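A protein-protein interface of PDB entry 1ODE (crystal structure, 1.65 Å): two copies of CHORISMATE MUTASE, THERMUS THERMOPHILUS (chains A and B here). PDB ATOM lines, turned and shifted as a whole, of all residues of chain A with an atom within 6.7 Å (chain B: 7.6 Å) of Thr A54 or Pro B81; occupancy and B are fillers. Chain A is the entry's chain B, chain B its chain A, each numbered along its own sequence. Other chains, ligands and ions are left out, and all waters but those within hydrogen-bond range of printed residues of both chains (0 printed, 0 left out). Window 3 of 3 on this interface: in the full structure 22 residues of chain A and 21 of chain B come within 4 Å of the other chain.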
ATOM      1  N   ASP A  14      13.769  12.794  26.359  1.00  0.00           N
ATOM      2  CA  ASP A  14      13.404  11.422  26.031  1.00  0.00           C
ATOM      3  C   ASP A  14      12.043  11.303  25.347  1.00  0.00           C
ATOM      4  O   ASP A  14      11.027  11.048  25.994  1.00  0.00           O
ATOM      5  CB  ASP A  14      13.438  10.568  27.304  1.00  0.00           C
ATOM      6  CG  ASP A  14      13.245   9.085  27.029  1.00  0.00           C
ATOM      7  OD1 ASP A  14      13.382   8.670  25.861  1.00  0.00           O
ATOM      8  OD2 ASP A  14      12.970   8.332  27.989  1.00  0.00           O
ATOM      9  N   ILE A  19      14.675  11.389  19.676  1.00  0.00           N
ATOM     10  CA  ILE A  19      15.613  10.290  19.492  1.00  0.00           C
ATOM     11  C   ILE A  19      15.801   9.981  18.012  1.00  0.00           C
ATOM     12  O   ILE A  19      16.928   9.851  17.538  1.00  0.00           O
ATOM     13  CB  ILE A  19      15.126   9.017  20.225  1.00  0.00           C
ATOM     14  CG1 ILE A  19      15.196   9.241  21.737  1.00  0.00           C
ATOM     15  CG2 ILE A  19      15.966   7.810  19.810  1.00  0.00           C
ATOM     16  CD1 ILE A  19      14.708   8.065  22.559  1.00  0.00           C
ATOM     17  N   VAL A  49      22.195   3.095  23.895  1.00  0.00           N
ATOM     18  CA  VAL A  49      21.566   4.295  24.414  1.00  0.00           C
ATOM     19  C   VAL A  49      21.708   4.282  25.925  1.00  0.00           C
ATOM     20  O   VAL A  49      21.676   3.223  26.542  1.00  0.00           O
ATOM     21  CB  VAL A  49      20.065   4.342  24.039  1.00  0.00           C
ATOM     22  CG1 VAL A  49      19.902   4.265  22.534  1.00  0.00           C
ATOM     23  CG2 VAL A  49      19.321   3.206  24.713  1.00  0.00           C
ATOM     24  N   THR A  50      21.887   5.460  26.516  1.00  0.00           N
ATOM     25  CA  THR A  50      22.016   5.561  27.961  1.00  0.00           C
ATOM     26  C   THR A  50      20.653   5.253  28.581  1.00  0.00           C
ATOM     27  O   THR A  50      19.622   5.352  27.911  1.00  0.00           O
ATOM     28  CB  THR A  50      22.488   6.969  28.362  1.00  0.00           C
ATOM     29  OG1 THR A  50      21.706   7.943  27.669  1.00  0.00           O
ATOM     30  CG2 THR A  50      23.953   7.159  27.993  1.00  0.00           C
ATOM     31  N   GLU A  51      20.647   4.875  29.855  1.00  0.00           N
ATOM     32  CA  GLU A  51      19.412   4.518  30.538  1.00  0.00           C
ATOM     33  C   GLU A  51      18.371   5.624  30.669  1.00  0.00           C
ATOM     34  O   GLU A  51      17.204   5.337  30.940  1.00  0.00           O
ATOM     35  CB  GLU A  51      19.718   3.938  31.923  1.00  0.00           C
ATOM     36  CG  GLU A  51      20.517   4.845  32.838  1.00  0.00           C
ATOM     37  CD  GLU A  51      20.645   4.274  34.236  1.00  0.00           C
ATOM     38  OE1 GLU A  51      21.113   3.123  34.370  1.00  0.00           O
ATOM     39  OE2 GLU A  51      20.275   4.974  35.203  1.00  0.00           O
ATOM     40  N   ASP A  52      18.770   6.879  30.485  1.00  0.00           N
ATOM     41  CA  ASP A  52      17.805   7.968  30.587  1.00  0.00           C
ATOM     42  C   ASP A  52      16.993   8.114  29.308  1.00  0.00           C
ATOM     43  O   ASP A  52      16.156   9.008  29.199  1.00  0.00           O
ATOM     44  CB  ASP A  52      18.495   9.298  30.919  1.00  0.00           C
ATOM     45  CG  ASP A  52      19.754   9.527  30.116  1.00  0.00           C
ATOM     46  OD1 ASP A  52      19.810   9.087  28.950  1.00  0.00           O
ATOM     47  OD2 ASP A  52      20.687  10.163  30.651  1.00  0.00           O
ATOM     48  N   LEU A  53      17.247   7.235  28.341  1.00  0.00           N
ATOM     49  CA  LEU A  53      16.518   7.250  27.075  1.00  0.00           C
ATOM     50  C   LEU A  53      15.855   5.894  26.870  1.00  0.00           C
ATOM     51  O   LEU A  53      16.526   4.906  26.560  1.00  0.00           O
ATOM     52  CB  LEU A  53      17.464   7.538  25.908  1.00  0.00           C
ATOM     53  CG  LEU A  53      18.085   8.930  25.814  1.00  0.00           C
ATOM     54  CD1 LEU A  53      19.079   8.972  24.661  1.00  0.00           C
ATOM     55  CD2 LEU A  53      16.988   9.960  25.614  1.00  0.00           C
ATOM     56  N   THR A  54      14.537   5.847  27.039  1.00  0.00           N
ATOM     57  CA  THR A  54      13.810   4.593  26.885  1.00  0.00           C
ATOM     58  C   THR A  54      12.501   4.734  26.117  1.00  0.00           C
ATOM     59  O   THR A  54      11.746   3.770  25.992  1.00  0.00           O
ATOM     60  CB  THR A  54      13.495   3.974  28.263  1.00  0.00           C
ATOM     61  OG1 THR A  54      12.723   4.902  29.035  1.00  0.00           O
ATOM     62  CG2 THR A  54      14.783   3.651  29.011  1.00  0.00           C
ATOM     63  N   SER A  55      12.239   5.922  25.583  1.00  0.00           N
ATOM     64  CA  SER A  55      10.995   6.161  24.856  1.00  0.00           C
ATOM     65  C   SER A  55      10.939   5.589  23.440  1.00  0.00           C
ATOM     66  O   SER A  55       9.853   5.433  22.882  1.00  0.00           O
ATOM     67  CB  SER A  55      10.690   7.663  24.803  1.00  0.00           C
ATOM     68  OG  SER A  55      11.633   8.355  24.003  1.00  0.00           O
ATOM     69  N   ALA A  56      12.091   5.278  22.856  1.00  0.00           N
ATOM     70  CA  ALA A  56      12.103   4.741  21.500  1.00  0.00           C
ATOM     71  C   ALA A  56      13.395   4.020  21.145  1.00  0.00           C
ATOM     72  O   ALA A  56      14.401   4.143  21.844  1.00  0.00           O
ATOM     73  CB  ALA A  56      11.855   5.865  20.500  1.00  0.00           C
ATOM     74  N   PHE A  57      13.344   3.263  20.052  1.00  0.00           N
ATOM     75  CA  PHE A  57      14.502   2.531  19.555  1.00  0.00           C
ATOM     76  C   PHE A  57      15.170   3.382  18.478  1.00  0.00           C
ATOM     77  O   PHE A  57      14.528   3.776  17.505  1.00  0.00           O
ATOM     78  CB  PHE A  57      14.076   1.198  18.936  1.00  0.00           C
ATOM     79  CG  PHE A  57      13.607   0.182  19.930  1.00  0.00           C
ATOM     80  CD1 PHE A  57      14.480  -0.330  20.884  1.00  0.00           C
ATOM     81  CD2 PHE A  57      12.295  -0.286  19.900  1.00  0.00           C
ATOM     82  CE1 PHE A  57      14.055  -1.299  21.794  1.00  0.00           C
ATOM     83  CE2 PHE A  57      11.861  -1.253  20.804  1.00  0.00           C
ATOM     84  CZ  PHE A  57      12.743  -1.761  21.753  1.00  0.00           C
ATOM     85  N   VAL B  78      17.502  -2.371  24.796  1.00  0.00           N
ATOM     86  CA  VAL B  78      16.996  -1.128  25.373  1.00  0.00           C
ATOM     87  C   VAL B  78      15.576  -1.372  25.888  1.00  0.00           C
ATOM     88  O   VAL B  78      14.696  -1.767  25.127  1.00  0.00           O
ATOM     89  CB  VAL B  78      16.951  -0.009  24.316  1.00  0.00           C
ATOM     90  CG1 VAL B  78      16.468   1.294  24.948  1.00  0.00           C
ATOM     91  CG2 VAL B  78      18.324   0.162  23.686  1.00  0.00           C
ATOM     92  N   PRO B  79      15.334  -1.127  27.187  1.00  0.00           N
ATOM     93  CA  PRO B  79      14.020  -1.324  27.810  1.00  0.00           C
ATOM     94  C   PRO B  79      12.956  -0.295  27.429  1.00  0.00           C
ATOM     95  O   PRO B  79      12.588   0.555  28.243  1.00  0.00           O
ATOM     96  CB  PRO B  79      14.346  -1.283  29.297  1.00  0.00           C
ATOM     97  CG  PRO B  79      15.436  -0.266  29.352  1.00  0.00           C
ATOM     98  CD  PRO B  79      16.318  -0.663  28.183  1.00  0.00           C
ATOM     99  N   VAL B  80      12.458  -0.376  26.200  1.00  0.00           N
ATOM    100  CA  VAL B  80      11.432   0.549  25.734  1.00  0.00           C
ATOM    101  C   VAL B  80      10.051   0.061  26.156  1.00  0.00           C
ATOM    102  O   VAL B  80       9.568  -0.964  25.673  1.00  0.00           O
ATOM    103  CB  VAL B  80      11.464   0.698  24.198  1.00  0.00           C
ATOM    104  CG1 VAL B  80      10.330   1.599  23.733  1.00  0.00           C
ATOM    105  CG2 VAL B  80      12.805   1.276  23.768  1.00  0.00           C
ATOM    106  N   PRO B  81       9.397   0.791  27.072  1.00  0.00           N
ATOM    107  CA  PRO B  81       8.064   0.403  27.541  1.00  0.00           C
ATOM    108  C   PRO B  81       7.094   0.189  26.383  1.00  0.00           C
ATOM    109  O   PRO B  81       7.086   0.956  25.421  1.00  0.00           O
ATOM    110  CB  PRO B  81       7.656   1.579  28.426  1.00  0.00           C
ATOM    111  CG  PRO B  81       8.967   2.059  28.972  1.00  0.00           C
ATOM    112  CD  PRO B  81       9.854   2.019  27.748  1.00  0.00           C
ATOM    113  N   GLY B  82       6.290  -0.863  26.477  1.00  0.00           N
ATOM    114  CA  GLY B  82       5.319  -1.143  25.435  1.00  0.00           C
ATOM    115  C   GLY B  82       5.847  -1.949  24.263  1.00  0.00           C
ATOM    116  O   GLY B  82       5.086  -2.297  23.362  1.00  0.00           O
ATOM    117  N   SER B  83       7.142  -2.250  24.261  1.00  0.00           N
ATOM    118  CA  SER B  83       7.715  -3.025  23.167  1.00  0.00           C
ATOM    119  C   SER B  83       7.396  -4.508  23.343  1.00  0.00           C
ATOM    120  O   SER B  83       6.991  -4.942  24.422  1.00  0.00           O
ATOM    121  CB  SER B  83       9.233  -2.807  23.093  1.00  0.00           C
ATOM    122  OG  SER B  83       9.869  -3.137  24.315  1.00  0.00           O
ATOM    123  N   LEU B  84       7.575  -5.276  22.272  1.00  0.00           N
ATOM    124  CA  LEU B  84       7.311  -6.713  22.287  1.00  0.00           C
ATOM    125  C   LEU B  84       8.037  -7.358  23.465  1.00  0.00           C
ATOM    126  O   LEU B  84       9.237  -7.180  23.637  1.00  0.00           O
ATOM    127  CB  LEU B  84       7.789  -7.338  20.974  1.00  0.00           C
ATOM    128  CG  LEU B  84       7.419  -8.791  20.663  1.00  0.00           C
ATOM    129  CD1 LEU B  84       5.916  -8.910  20.453  1.00  0.00           C
ATOM    130  CD2 LEU B  84       8.164  -9.244  19.411  1.00  0.00           C
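The backbone NH (N) of Thr A54 lies within hydrogen-bond range of the side-chain carboxylate (OD2) of Asp A14 (3.1 Å). The side-chain hydroxyl (OG) of Ser A55 lies within hydrogen-bond range of the side-chain carboxylate (OD1) of Asp A14. O of Val B80 sits at hydrogen-bond distance from OG of Ser B83 (2.6 Å).
CG2 of Val A49 touches CG2 of Val B78, at 3.4 Å. CG1 of Val B78 touches O of Leu A53, 3.96 Å away. Pro B79 touches Thr A54. CA of Val B80 touches O of Thr A54, at 3.2 Å. Thr A54 touches Pro B81. O of Ser A55 touches CG1 of Val B80, at 3.96 Å. O of Ala A56 touches CG2 of Val B80, at 3.8 Å. Phe A57 touches Val B78. CG2 of Val B80 touches CE1 of Phe A57, at 3.5 Å. Phe A57 touches Ser B83 (CE2 to CB, 3.8 Å).
Thr A54 touches just these residues of chain B: Pro B79, Val B80 and Pro B81. Pro B81 touches just one residue of chain A: Thr A54 (3.1 Å). Printed residues of chain A within 4 Å of Val B80: Thr A54, Ser A55, Ala A56 and Phe A57. Of the printed residues of chain A, Pro B79 touches Thr A54. Ile A19 touches none of the printed residues of chain B. The nearest residue of chain A that does not touch Pro B81 is Ser A55 (5.1 Å). The nearest printed residue of chain B that does not touch Ser A55 is Pro B81 (5.1 Å).
Of the 11 printed residues of chain A, 6 touch a printed residue of chain B. Hydrophobic or aromatic side chains of chain A within 4 Å of the printed part of chain B: Val A49 and Phe A57. Printed residues of chain B that touch a printed residue of chain A: Val B78, Pro B79, Val B80, Pro B81 and Ser B83. Along chain B the printed residues that touch a printed residue of chain A span positions 78 to 83. Among the printed residues, no Asp or Glu carboxylate lies within 4 Å of a Lys or Arg side-chain nitrogen of the other chain.
No position is printed for both chains. Of the 10 pairs that touch across the chains among the printed residues, none has its exchanged pair printed and touching as well.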
